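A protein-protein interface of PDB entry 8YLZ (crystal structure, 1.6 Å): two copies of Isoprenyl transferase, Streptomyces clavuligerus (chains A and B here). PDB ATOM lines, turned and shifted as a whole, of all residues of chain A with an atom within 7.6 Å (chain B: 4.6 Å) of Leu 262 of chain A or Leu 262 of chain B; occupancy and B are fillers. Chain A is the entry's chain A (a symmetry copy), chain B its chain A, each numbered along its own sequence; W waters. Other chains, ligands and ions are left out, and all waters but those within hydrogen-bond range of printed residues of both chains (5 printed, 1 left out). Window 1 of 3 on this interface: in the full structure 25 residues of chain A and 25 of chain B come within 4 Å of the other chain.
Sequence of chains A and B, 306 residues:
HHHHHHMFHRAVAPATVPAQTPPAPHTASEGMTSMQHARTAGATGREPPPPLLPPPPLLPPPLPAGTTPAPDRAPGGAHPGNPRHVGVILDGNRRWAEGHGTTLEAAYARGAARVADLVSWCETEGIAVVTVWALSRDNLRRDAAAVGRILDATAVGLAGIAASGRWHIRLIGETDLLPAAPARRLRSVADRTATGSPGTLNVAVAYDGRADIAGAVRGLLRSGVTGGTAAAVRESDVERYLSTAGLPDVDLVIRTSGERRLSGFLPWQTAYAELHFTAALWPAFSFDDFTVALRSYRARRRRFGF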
ATOM      1  N   GLY A  87       0.565 -24.525  20.712  1.00  0.00           N
ATOM      2  CA  GLY A  87      -0.217 -23.311  20.483  1.00  0.00           C
ATOM      3  C   GLY A  87      -0.229 -23.029  18.992  1.00  0.00           C
ATOM      4  O   GLY A  87       0.802 -23.124  18.332  1.00  0.00           O
ATOM      5  N   ILE A  89      -1.564 -20.282  16.023  1.00  0.00           N
ATOM      6  CA  ILE A  89      -2.131 -18.984  15.668  1.00  0.00           C
ATOM      7  C   ILE A  89      -2.863 -19.171  14.340  1.00  0.00           C
ATOM      8  O   ILE A  89      -2.233 -19.447  13.314  1.00  0.00           O
ATOM      9  CB  ILE A  89      -1.044 -17.906  15.606  1.00  0.00           C
ATOM     10  CG1 ILE A  89      -0.305 -17.832  16.951  1.00  0.00           C
ATOM     11  CG2 ILE A  89      -1.666 -16.547  15.216  1.00  0.00           C
ATOM     12  CD1 ILE A  89       0.934 -16.920  16.894  1.00  0.00           C
ATOM     13  N   TRP A 133      -5.353 -19.558  18.833  1.00  0.00           N
ATOM     14  CA  TRP A 133      -5.686 -18.140  18.835  1.00  0.00           C
ATOM     15  C   TRP A 133      -6.576 -17.864  17.630  1.00  0.00           C
ATOM     16  O   TRP A 133      -6.106 -17.843  16.490  1.00  0.00           O
ATOM     17  CB  TRP A 133      -4.420 -17.287  18.803  1.00  0.00           C
ATOM     18  CG  TRP A 133      -4.668 -15.825  19.073  1.00  0.00           C
ATOM     19  CD1 TRP A 133      -5.833 -15.245  19.469  1.00  0.00           C
ATOM     20  CD2 TRP A 133      -3.704 -14.774  18.968  1.00  0.00           C
ATOM     21  NE1 TRP A 133      -5.645 -13.879  19.612  1.00  0.00           N
ATOM     22  CE2 TRP A 133      -4.347 -13.580  19.314  1.00  0.00           C
ATOM     23  CE3 TRP A 133      -2.340 -14.743  18.633  1.00  0.00           C
ATOM     24  CZ2 TRP A 133      -3.694 -12.361  19.319  1.00  0.00           C
ATOM     25  CZ3 TRP A 133      -1.691 -13.523  18.611  1.00  0.00           C
ATOM     26  CH2 TRP A 133      -2.372 -12.346  18.954  1.00  0.00           C
ATOM     27  N   TYR A 207      -8.108 -11.789  22.446  1.00  0.00           N
ATOM     28  CA  TYR A 207      -6.902 -11.939  23.254  1.00  0.00           C
ATOM     29  C   TYR A 207      -5.818 -11.004  22.746  1.00  0.00           C
ATOM     30  O   TYR A 207      -5.713 -10.770  21.545  1.00  0.00           O
ATOM     31  CB  TYR A 207      -6.378 -13.384  23.210  1.00  0.00           C
ATOM     32  CG  TYR A 207      -5.071 -13.531  23.926  1.00  0.00           C
ATOM     33  CD1 TYR A 207      -5.030 -13.700  25.296  1.00  0.00           C
ATOM     34  CD2 TYR A 207      -3.865 -13.423  23.232  1.00  0.00           C
ATOM     35  CE1 TYR A 207      -3.841 -13.796  25.962  1.00  0.00           C
ATOM     36  CE2 TYR A 207      -2.681 -13.486  23.883  1.00  0.00           C
ATOM     37  CZ  TYR A 207      -2.666 -13.692  25.246  1.00  0.00           C
ATOM     38  OH  TYR A 207      -1.445 -13.760  25.882  1.00  0.00           O
ATOM     39  N   VAL A 253       4.885 -23.492  18.972  1.00  0.00           N
ATOM     40  CA  VAL A 253       3.922 -22.575  18.374  1.00  0.00           C
ATOM     41  C   VAL A 253       3.939 -22.801  16.871  1.00  0.00           C
ATOM     42  O   VAL A 253       5.013 -22.897  16.272  1.00  0.00           O
ATOM     43  CB  VAL A 253       4.268 -21.113  18.694  1.00  0.00           C
ATOM     44  CG1 VAL A 253       3.396 -20.171  17.858  1.00  0.00           C
ATOM     45  CG2 VAL A 253       4.187 -20.802  20.193  1.00  0.00           C
ATOM     46  N   ILE A 254       2.760 -22.900  16.273  1.00  0.00           N
ATOM     47  CA  ILE A 254       2.597 -22.975  14.833  1.00  0.00           C
ATOM     48  C   ILE A 254       1.834 -21.735  14.426  1.00  0.00           C
ATOM     49  O   ILE A 254       0.799 -21.437  15.017  1.00  0.00           O
ATOM     50  CB  ILE A 254       1.822 -24.236  14.427  1.00  0.00           C
ATOM     51  CG1 ILE A 254       2.541 -25.512  14.898  1.00  0.00           C
ATOM     52  CG2 ILE A 254       1.563 -24.201  12.918  1.00  0.00           C
ATOM     53  CD1 ILE A 254       1.669 -26.742  14.701  1.00  0.00           C
ATOM     54  N   ARG A 255       2.337 -20.991  13.445  1.00  0.00           N
ATOM     55  CA  ARG A 255       1.549 -19.914  12.868  1.00  0.00           C
ATOM     56  C   ARG A 255       1.445 -20.145  11.375  1.00  0.00           C
ATOM     57  O   ARG A 255       2.460 -20.385  10.709  1.00  0.00           O
ATOM     58  CB  ARG A 255       2.128 -18.533  13.118  1.00  0.00           C
ATOM     59  CG  ARG A 255       1.206 -17.473  12.491  1.00  0.00           C
ATOM     60  CD  ARG A 255       1.497 -16.144  13.055  1.00  0.00           C
ATOM     61  NE  ARG A 255       0.675 -15.104  12.457  1.00  0.00           N
ATOM     62  CZ  ARG A 255       0.597 -13.890  12.976  1.00  0.00           C
ATOM     63  NH1 ARG A 255       1.327 -13.548  14.030  1.00  0.00           N
ATOM     64  NH2 ARG A 255      -0.259 -13.009  12.454  1.00  0.00           N
ATOM     65  N   GLU A 259       3.189 -15.871   7.895  1.00  0.00           N
ATOM     66  CA  GLU A 259       3.551 -14.730   8.731  1.00  0.00           C
ATOM     67  C   GLU A 259       4.544 -15.162   9.794  1.00  0.00           C
ATOM     68  O   GLU A 259       4.214 -15.984  10.654  1.00  0.00           O
ATOM     69  CB  GLU A 259       2.300 -14.156   9.383  1.00  0.00           C
ATOM     70  CG  GLU A 259       2.525 -12.884  10.140  1.00  0.00           C
ATOM     71  CD  GLU A 259       2.373 -11.665   9.260  1.00  0.00           C
ATOM     72  OE1 GLU A 259       2.387 -10.541   9.800  1.00  0.00           O
ATOM     73  OE2 GLU A 259       2.234 -11.839   8.024  1.00  0.00           O
ATOM     74  N   ARG A 260       5.712 -14.530   9.811  1.00  0.00           N
ATOM     75  CA  ARG A 260       6.797 -14.956  10.700  1.00  0.00           C
ATOM     76  C   ARG A 260       6.847 -14.057  11.931  1.00  0.00           C
ATOM     77  O   ARG A 260       7.825 -13.357  12.198  1.00  0.00           O
ATOM     78  CB  ARG A 260       8.117 -14.946   9.943  1.00  0.00           C
ATOM     79  CG  ARG A 260       8.115 -15.919   8.780  1.00  0.00           C
ATOM     80  CD  ARG A 260       9.486 -15.998   8.173  1.00  0.00           C
ATOM     81  NE  ARG A 260      10.438 -16.461   9.173  1.00  0.00           N
ATOM     82  CZ  ARG A 260      10.593 -17.733   9.511  1.00  0.00           C
ATOM     83  NH1 ARG A 260       9.943 -18.700   8.880  1.00  0.00           N
ATOM     84  NH2 ARG A 260      11.426 -18.045  10.503  1.00  0.00           N
ATOM     85  N   ARG A 261       5.738 -14.062  12.670  1.00  0.00           N
ATOM     86  CA  ARG A 261       5.571 -13.174  13.811  1.00  0.00           C
ATOM     87  C   ARG A 261       4.751 -13.902  14.860  1.00  0.00           C
ATOM     88  O   ARG A 261       3.931 -14.761  14.524  1.00  0.00           O
ATOM     89  CB  ARG A 261       4.847 -11.886  13.414  1.00  0.00           C
ATOM     90  CG  ARG A 261       5.653 -10.987  12.510  1.00  0.00           C
ATOM     91  CD  ARG A 261       5.126  -9.585  12.600  1.00  0.00           C
ATOM     92  NE  ARG A 261       3.741  -9.484  12.174  1.00  0.00           N
ATOM     93  CZ  ARG A 261       3.174  -8.349  11.793  1.00  0.00           C
ATOM     94  NH1 ARG A 261       3.835  -7.203  11.828  1.00  0.00           N
ATOM     95  NH2 ARG A 261       1.910  -8.361  11.378  1.00  0.00           N
ATOM     96  N   LEU A 262       4.948 -13.546  16.130  1.00  0.00           N
ATOM     97  CA  LEU A 262       4.110 -14.093  17.192  1.00  0.00           C
ATOM     98  C   LEU A 262       2.919 -13.192  17.501  1.00  0.00           C
ATOM     99  O   LEU A 262       1.895 -13.676  17.996  1.00  0.00           O
ATOM    100  CB  LEU A 262       4.962 -14.296  18.466  1.00  0.00           C
ATOM    101  CG  LEU A 262       5.727 -15.577  18.807  1.00  0.00           C
ATOM    102  CD1 LEU A 262       6.611 -15.368  20.052  1.00  0.00           C
ATOM    103  CD2 LEU A 262       4.766 -16.716  19.075  1.00  0.00           C
ATOM    104  N   SER A 263       3.023 -11.894  17.202  1.00  0.00           N
ATOM    105  CA  SER A 263       1.954 -10.917  17.436  1.00  0.00           C
ATOM    106  C   SER A 263       1.474 -10.923  18.881  1.00  0.00           C
ATOM    107  O   SER A 263       0.306 -10.640  19.152  1.00  0.00           O
ATOM    108  CB  SER A 263       0.777 -11.121  16.479  1.00  0.00           C
ATOM    109  OG  SER A 263       1.248 -10.984  15.149  1.00  0.00           O
ATOM    110  N   GLY A 264       2.400 -11.170  19.811  1.00  0.00           N
ATOM    111  CA  GLY A 264       2.051 -11.145  21.219  1.00  0.00           C
ATOM    112  C   GLY A 264       1.259 -12.332  21.714  1.00  0.00           C
ATOM    113  O   GLY A 264       0.562 -12.213  22.720  1.00  0.00           O
ATOM    114  N   PHE A 265       1.298 -13.461  21.019  1.00  0.00           N
ATOM    115  CA  PHE A 265       0.619 -14.675  21.488  1.00  0.00           C
ATOM    116  C   PHE A 265       1.286 -15.209  22.759  1.00  0.00           C
ATOM    117  O   PHE A 265       2.431 -15.672  22.718  1.00  0.00           O
ATOM    118  CB  PHE A 265       0.672 -15.715  20.371  1.00  0.00           C
ATOM    119  CG  PHE A 265       0.010 -17.028  20.665  1.00  0.00           C
ATOM    120  CD1 PHE A 265      -1.303 -17.115  21.095  1.00  0.00           C
ATOM    121  CD2 PHE A 265       0.724 -18.198  20.468  1.00  0.00           C
ATOM    122  CE1 PHE A 265      -1.893 -18.361  21.307  1.00  0.00           C
ATOM    123  CE2 PHE A 265       0.156 -19.442  20.688  1.00  0.00           C
ATOM    124  CZ  PHE A 265      -1.157 -19.532  21.112  1.00  0.00           C
ATOM    125  N   LEU A 266       0.547 -15.202  23.882  1.00  0.00           N
ATOM    126  CA  LEU A 266       1.031 -15.767  25.151  1.00  0.00           C
ATOM    127  C   LEU A 266       2.505 -15.454  25.403  1.00  0.00           C
ATOM    128  O   LEU A 266       3.348 -16.365  25.468  1.00  0.00           O
ATOM    129  CB  LEU A 266       0.800 -17.277  25.187  1.00  0.00           C
ATOM    130  CG  LEU A 266      -0.651 -17.742  25.018  1.00  0.00           C
ATOM    131  CD1 LEU A 266      -0.659 -19.224  24.908  1.00  0.00           C
ATOM    132  CD2 LEU A 266      -1.442 -17.279  26.225  1.00  0.00           C
ATOM    133  N   PRO A 267       2.853 -14.180  25.588  1.00  0.00           N
ATOM    134  CA  PRO A 267       4.283 -13.834  25.707  1.00  0.00           C
ATOM    135  C   PRO A 267       4.978 -14.571  26.836  1.00  0.00           C
ATOM    136  O   PRO A 267       6.137 -14.978  26.684  1.00  0.00           O
ATOM    137  CB  PRO A 267       4.264 -12.320  25.935  1.00  0.00           C
ATOM    138  CG  PRO A 267       2.832 -11.965  26.250  1.00  0.00           C
ATOM    139  CD  PRO A 267       1.963 -13.003  25.675  1.00  0.00           C
ATOM    140  N   THR A 270       5.135 -18.691  25.942  1.00  0.00           N
ATOM    141  CA  THR A 270       5.852 -19.065  24.727  1.00  0.00           C
ATOM    142  C   THR A 270       7.306 -18.635  24.737  1.00  0.00           C
ATOM    143  O   THR A 270       7.992 -18.803  23.724  1.00  0.00           O
ATOM    144  CB  THR A 270       5.174 -18.488  23.475  1.00  0.00           C
ATOM    145  OG1 THR A 270       5.185 -17.052  23.537  1.00  0.00           O
ATOM    146  CG2 THR A 270       3.718 -19.020  23.325  1.00  0.00           C
ATOM    147  N   ALA A 271       7.801 -18.114  25.864  1.00  0.00           N
ATOM    148  CA  ALA A 271       9.153 -17.562  25.884  1.00  0.00           C
ATOM    149  C   ALA A 271      10.165 -18.561  25.352  1.00  0.00           C
ATOM    150  O   ALA A 271      11.091 -18.189  24.622  1.00  0.00           O
ATOM    151  CB  ALA A 271       9.520 -17.129  27.305  1.00  0.00           C
ATOM    152  N   TYR A 272      10.000 -19.841  25.691  1.00  0.00           N
ATOM    153  CA  TYR A 272      10.951 -20.864  25.276  1.00  0.00           C
ATOM    154  C   TYR A 272      10.352 -21.863  24.299  1.00  0.00           C
ATOM    155  O   TYR A 272      10.889 -22.958  24.111  1.00  0.00           O
ATOM    156  CB  TYR A 272      11.513 -21.576  26.507  1.00  0.00           C
ATOM    157  CG  TYR A 272      12.310 -20.631  27.370  1.00  0.00           C
ATOM    158  CD1 TYR A 272      13.657 -20.403  27.125  1.00  0.00           C
ATOM    159  CD2 TYR A 272      11.708 -19.951  28.420  1.00  0.00           C
ATOM    160  CE1 TYR A 272      14.391 -19.534  27.920  1.00  0.00           C
ATOM    161  CE2 TYR A 272      12.432 -19.073  29.211  1.00  0.00           C
ATOM    162  CZ  TYR A 272      13.771 -18.870  28.949  1.00  0.00           C
ATOM    163  OH  TYR A 272      14.503 -17.998  29.730  1.00  0.00           O
ATOM    164  N   ALA A 273       9.258 -21.498  23.650  1.00  0.00           N
ATOM    165  CA  ALA A 273       8.648 -22.379  22.673  1.00  0.00           C
ATOM    166  C   ALA A 273       9.460 -22.422  21.383  1.00  0.00           C
ATOM    167  O   ALA A 273      10.001 -21.404  20.935  1.00  0.00           O
ATOM    168  CB  ALA A 273       7.232 -21.901  22.372  1.00  0.00           C
ATOM    169  N   GLU A 274       9.508 -23.609  20.777  1.00  0.00           N
ATOM    170  CA  GLU A 274       9.917 -23.753  19.387  1.00  0.00           C
ATOM    171  C   GLU A 274       8.897 -23.063  18.495  1.00  0.00           C
ATOM    172  O   GLU A 274       7.691 -23.228  18.689  1.00  0.00           O
ATOM    173  CB  GLU A 274       9.998 -25.234  19.037  1.00  0.00           C
ATOM    174  CG  GLU A 274      10.362 -25.539  17.612  1.00  0.00           C
ATOM    175  CD  GLU A 274      11.859 -25.480  17.376  1.00  0.00           C
ATOM    176  OE1 GLU A 274      12.622 -25.393  18.365  1.00  0.00           O
ATOM    177  OE2 GLU A 274      12.267 -25.570  16.195  1.00  0.00           O
ATOM    178  N   LEU A 275       9.366 -22.294  17.517  1.00  0.00           N
ATOM    179  CA  LEU A 275       8.471 -21.494  16.684  1.00  0.00           C
ATOM    180  C   LEU A 275       8.490 -22.011  15.257  1.00  0.00           C
ATOM    181  O   LEU A 275       9.536 -21.976  14.602  1.00  0.00           O
ATOM    182  CB  LEU A 275       8.898 -20.020  16.716  1.00  0.00           C
ATOM    183  CG  LEU A 275       9.025 -19.416  18.123  1.00  0.00           C
ATOM    184  CD1 LEU A 275       9.478 -17.955  17.981  1.00  0.00           C
ATOM    185  CD2 LEU A 275       7.705 -19.477  18.896  1.00  0.00           C
ATOM    186  N   PHE A 277       6.700 -21.895  11.365  1.00  0.00           N
ATOM    187  CA  PHE A 277       5.883 -21.079  10.485  1.00  0.00           C
ATOM    188  C   PHE A 277       5.460 -21.912   9.282  1.00  0.00           C
ATOM    189  O   PHE A 277       6.310 -22.432   8.552  1.00  0.00           O
ATOM    190  CB  PHE A 277       6.664 -19.821  10.100  1.00  0.00           C
ATOM    191  CG  PHE A 277       6.961 -18.948  11.290  1.00  0.00           C
ATOM    192  CD1 PHE A 277       5.927 -18.456  12.057  1.00  0.00           C
ATOM    193  CD2 PHE A 277       8.262 -18.714  11.695  1.00  0.00           C
ATOM    194  CE1 PHE A 277       6.172 -17.690  13.193  1.00  0.00           C
ATOM    195  CE2 PHE A 277       8.523 -17.947  12.823  1.00  0.00           C
ATOM    196  CZ  PHE A 277       7.483 -17.437  13.571  1.00  0.00           C
ATOM    197  N   ILE B  89      19.962 -12.095  18.523  1.00  0.00           N
ATOM    198  CA  ILE B  89      20.296 -13.006  19.615  1.00  0.00           C
ATOM    199  C   ILE B  89      21.578 -13.733  19.206  1.00  0.00           C
ATOM    200  O   ILE B  89      21.577 -14.503  18.241  1.00  0.00           O
ATOM    201  CB  ILE B  89      19.136 -13.961  19.911  1.00  0.00           C
ATOM    202  CG1 ILE B  89      17.868 -13.157  20.238  1.00  0.00           C
ATOM    203  CG2 ILE B  89      19.519 -14.922  21.058  1.00  0.00           C
ATOM    204  CD1 ILE B  89      16.614 -14.045  20.339  1.00  0.00           C
ATOM    205  N   TRP B 133      21.736  -9.467  22.090  1.00  0.00           N
ATOM    206  CA  TRP B 133      21.677 -10.234  23.327  1.00  0.00           C
ATOM    207  C   TRP B 133      22.925 -11.104  23.402  1.00  0.00           C
ATOM    208  O   TRP B 133      23.041 -12.101  22.685  1.00  0.00           O
ATOM    209  CB  TRP B 133      20.403 -11.074  23.384  1.00  0.00           C
ATOM    210  CG  TRP B 133      20.139 -11.683  24.736  1.00  0.00           C
ATOM    211  CD1 TRP B 133      20.812 -11.446  25.895  1.00  0.00           C
ATOM    212  CD2 TRP B 133      19.109 -12.625  25.049  1.00  0.00           C
ATOM    213  NE1 TRP B 133      20.256 -12.200  26.916  1.00  0.00           N
ATOM    214  CE2 TRP B 133      19.211 -12.920  26.413  1.00  0.00           C
ATOM    215  CE3 TRP B 133      18.089 -13.228  24.294  1.00  0.00           C
ATOM    216  CZ2 TRP B 133      18.357 -13.804  27.048  1.00  0.00           C
ATOM    217  CZ3 TRP B 133      17.250 -14.132  24.918  1.00  0.00           C
ATOM    218  CH2 TRP B 133      17.390 -14.410  26.287  1.00  0.00           C
ATOM    219  N   VAL B 253      13.870  -9.479  14.446  1.00  0.00           N
ATOM    220  CA  VAL B 253      14.746 -10.252  15.317  1.00  0.00           C
ATOM    221  C   VAL B 253      15.477 -11.270  14.456  1.00  0.00           C
ATOM    222  O   VAL B 253      14.858 -11.929  13.618  1.00  0.00           O
ATOM    223  CB  VAL B 253      13.951 -10.966  16.420  1.00  0.00           C
ATOM    224  CG1 VAL B 253      14.853 -11.958  17.161  1.00  0.00           C
ATOM    225  CG2 VAL B 253      13.257  -9.987  17.374  1.00  0.00           C
ATOM    226  N   ARG B 255      17.983 -14.583  15.022  1.00  0.00           N
ATOM    227  CA  ARG B 255      18.662 -15.477  15.945  1.00  0.00           C
ATOM    228  C   ARG B 255      19.492 -16.455  15.140  1.00  0.00           C
ATOM    229  O   ARG B 255      18.989 -17.065  14.189  1.00  0.00           O
ATOM    230  CB  ARG B 255      17.718 -16.253  16.848  1.00  0.00           C
ATOM    231  CG  ARG B 255      18.539 -17.144  17.797  1.00  0.00           C
ATOM    232  CD  ARG B 255      17.709 -17.578  18.934  1.00  0.00           C
ATOM    233  NE  ARG B 255      18.436 -18.459  19.835  1.00  0.00           N
ATOM    234  CZ  ARG B 255      17.971 -18.770  21.034  1.00  0.00           C
ATOM    235  NH1 ARG B 255      16.780 -18.346  21.437  1.00  0.00           N
ATOM    236  NH2 ARG B 255      18.730 -19.490  21.863  1.00  0.00           N
ATOM    237  N   ARG B 261      13.759 -20.143  18.402  1.00  0.00           N
ATOM    238  CA  ARG B 261      13.163 -19.762  19.674  1.00  0.00           C
ATOM    239  C   ARG B 261      13.557 -18.327  19.970  1.00  0.00           C
ATOM    240  O   ARG B 261      14.620 -17.871  19.538  1.00  0.00           O
ATOM    241  CB  ARG B 261      13.653 -20.662  20.811  1.00  0.00           C
ATOM    242  CG  ARG B 261      13.163 -22.084  20.717  1.00  0.00           C
ATOM    243  CD  ARG B 261      13.233 -22.727  22.071  1.00  0.00           C
ATOM    244  NE  ARG B 261      14.588 -22.779  22.591  1.00  0.00           N
ATOM    245  CZ  ARG B 261      14.974 -23.612  23.547  1.00  0.00           C
ATOM    246  NH1 ARG B 261      14.116 -24.430  24.134  1.00  0.00           N
ATOM    247  NH2 ARG B 261      16.247 -23.616  23.930  1.00  0.00           N
ATOM    248  N   LEU B 262      12.720 -17.617  20.727  1.00  0.00           N
ATOM    249  CA  LEU B 262      13.081 -16.277  21.175  1.00  0.00           C
ATOM    250  C   LEU B 262      13.739 -16.291  22.551  1.00  0.00           C
ATOM    251  O   LEU B 262      14.504 -15.377  22.876  1.00  0.00           O
ATOM    252  CB  LEU B 262      11.816 -15.387  21.206  1.00  0.00           C
ATOM    253  CG  LEU B 262      11.315 -14.544  20.031  1.00  0.00           C
ATOM    254  CD1 LEU B 262       9.937 -13.932  20.349  1.00  0.00           C
ATOM    255  CD2 LEU B 262      12.288 -13.426  19.723  1.00  0.00           C
ATOM    256  N   SER B 263      13.474 -17.321  23.359  1.00  0.00           N
ATOM    257  CA  SER B 263      14.044 -17.470  24.702  1.00  0.00           C
ATOM    258  C   SER B 263      13.792 -16.246  25.573  1.00  0.00           C
ATOM    259  O   SER B 263      14.598 -15.926  26.449  1.00  0.00           O
ATOM    260  CB  SER B 263      15.539 -17.795  24.654  1.00  0.00           C
ATOM    261  OG  SER B 263      15.715 -19.006  23.939  1.00  0.00           O
ATOM    262  N   GLY B 264      12.633 -15.612  25.381  1.00  0.00           N
ATOM    263  CA  GLY B 264      12.279 -14.466  26.198  1.00  0.00           C
ATOM    264  C   GLY B 264      13.015 -13.187  25.880  1.00  0.00           C
ATOM    265  O   GLY B 264      13.119 -12.321  26.747  1.00  0.00           O
ATOM    266  N   PHE B 265      13.573 -13.052  24.684  1.00  0.00           N
ATOM    267  CA  PHE B 265      14.231 -11.803  24.281  1.00  0.00           C
ATOM    268  C   PHE B 265      13.207 -10.674  24.143  1.00  0.00           C
ATOM    269  O   PHE B 265      12.359 -10.704  23.244  1.00  0.00           O
ATOM    270  CB  PHE B 265      14.951 -12.047  22.956  1.00  0.00           C
ATOM    271  CG  PHE B 265      15.699 -10.876  22.390  1.00  0.00           C
ATOM    272  CD1 PHE B 265      16.645 -10.179  23.122  1.00  0.00           C
ATOM    273  CD2 PHE B 265      15.461 -10.500  21.079  1.00  0.00           C
ATOM    274  CE1 PHE B 265      17.353  -9.129  22.537  1.00  0.00           C
ATOM    275  CE2 PHE B 265      16.146  -9.450  20.489  1.00  0.00           C
ATOM    276  CZ  PHE B 265      17.096  -8.755  21.216  1.00  0.00           C
ATOM    277  N   THR B 270       9.295  -7.088  21.157  1.00  0.00           N
ATOM    278  CA  THR B 270       9.331  -7.965  19.991  1.00  0.00           C
ATOM    279  C   THR B 270       7.979  -8.566  19.656  1.00  0.00           C
ATOM    280  O   THR B 270       7.899  -9.405  18.754  1.00  0.00           O
ATOM    281  CB  THR B 270      10.346  -9.103  20.177  1.00  0.00           C
ATOM    282  OG1 THR B 270       9.962  -9.918  21.296  1.00  0.00           O
ATOM    283  CG2 THR B 270      11.788  -8.548  20.371  1.00  0.00           C
ATOM    284  N   ALA B 271       6.913  -8.136  20.338  1.00  0.00           N
ATOM    285  CA  ALA B 271       5.615  -8.778  20.148  1.00  0.00           C
ATOM    286  C   ALA B 271       5.235  -8.831  18.678  1.00  0.00           C
ATOM    287  O   ALA B 271       4.689  -9.834  18.206  1.00  0.00           O
ATOM    288  CB  ALA B 271       4.544  -8.040  20.954  1.00  0.00           C
ATOM    289  N   LEU B 275      10.418 -12.390  12.643  1.00  0.00           N
ATOM    290  CA  LEU B 275      11.373 -13.289  13.288  1.00  0.00           C
ATOM    291  C   LEU B 275      12.137 -14.075  12.237  1.00  0.00           C
ATOM    292  O   LEU B 275      11.536 -14.848  11.487  1.00  0.00           O
ATOM    293  CB  LEU B 275      10.638 -14.250  14.232  1.00  0.00           C
ATOM    294  CG  LEU B 275       9.737 -13.567  15.273  1.00  0.00           C
ATOM    295  CD1 LEU B 275       9.062 -14.659  16.116  1.00  0.00           C
ATOM    296  CD2 LEU B 275      10.525 -12.621  16.183  1.00  0.00           C
HETATM  297  O   HOH W   1       6.786 -11.557  16.737  1.00  0.00           O
HETATM  298  O   HOH W   2       5.264 -11.988  20.686  1.00  0.00           O
HETATM  299  O   HOH W   3      12.635 -25.831  21.599  1.00  0.00           O
HETATM  300  O   HOH W   4      14.671 -14.691  28.767  1.00  0.00           O
HETATM  301  O   HOH W   5       9.981 -15.145  23.837  1.00  0.00           O
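Gly 87 of chain A touches none of the printed residues of chain B.
Ile 89 of chain A touches none of the printed residues of chain B.
Leu 262 of chain A touches just these residues of chain B: Leu 262 and Ala 271.
Printed residues of chain B within 4 Å of Ser 263 of chain A: Ala 271 (2.8 Å).
Of the printed residues of chain B, Ala 271 of chain A touches Leu 262, Ser 263 and Gly 264.
Of chain A, only Leu 262 (3.6 Å) and Ala 271 (3.9 Å) come within 4 Å of Leu 262 of chain B.
The nearest residue of chain B that does not touch Leu 262 of chain A is Leu 275 of chain B (4.3 Å).
The nearest residue of chain A that does not touch Leu 262 of chain B is Leu 275 of chain A (4.3 Å).
Ala 271 of chain A touches Leu 262 of chain B (O to C, 3.9 Å).
Tyr 272 of chain A touches Arg 261 of chain B.
Tyr 272 of chain A touches Ser 263 of chain B (CD1 to CA, 3.8 Å).
CG of Arg 261 of chain B touches O of Ala 273 of chain A, at 3.2 Å.
Glu 274 of chain A touches Arg 261 of chain B (CA to CG, 3.9 Å).
CD1 of Leu 275 of chain B touches CD1 of Leu 275 of chain A, 3.8 Å away.
Hydrophobic or aromatic side chains of chain B that line the printed part of chain A: Leu 262, Ala 271 and Leu 275.
Along chain A the printed residues that touch a printed residue of chain B span positions 260 to 275.
Among the printed residues, 13 pairs touch across the chains.
Water W1 lies within hydrogen-bond range of the backbone NH of Leu 262 of chain A (2.8 Å), the backbone carbonyl oxygen of Ala 271 of chain B (3.1 Å) and the backbone carbonyl oxygen of Thr 270 of chain B (3.2 Å).
Water W5 lies within hydrogen-bond range of the backbone NH of Gly 264 of chain B (3.1 Å) and the backbone carbonyl oxygen of Ala 271 of chain A (3.3 Å).
NH1 of Arg 255 of chain A is in hydrogen-bond range of OG of Ser 263 of chain A.
The guanidinium group (NH1) of Arg 255 of chain B is in hydrogen-bond range of the backbone carbonyl oxygen (O) of Arg 261 of chain B (2.9 Å).
The backbone NH of Val 253 of chain A is in hydrogen-bond range of the backbone carbonyl oxygen of Glu 274 of chain A.
Leu 262 of chain B touches its own counterpart, Leu 262 of chain A.
Leu 262 of chain A touches Ala 271 of chain B, and with the chains exchanged Ala 271 of chain A touches Leu 262 of chain B.
Ser 263 of chain A touches Ala 271 of chain B, and with the chains exchanged Ala 271 of chain A touches Ser 263 of chain B.
The backbone carbonyl oxygen (O) of Ala 271 of chain A sits at hydrogen-bond distance from the backbone NH (N) of Gly 264 of chain B, 3.1 Å away.
N of Ser 263 of chain A sits at hydrogen-bond distance from O of Ala 271 of chain B (2.8 Å).
The backbone NH (N) of Gly 264 of chain A sits at hydrogen-bond distance from the backbone carbonyl oxygen (O) of Ala 271 of chain B, at 3.1 Å.
The backbone carbonyl oxygen of Arg 260 of chain A lies within hydrogen-bond range of the backbone NH of Leu 275 of chain B (2.8 Å).
N of Ser 263 of chain B sits at hydrogen-bond distance from O of Ala 271 of chain A, 2.8 Å away.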
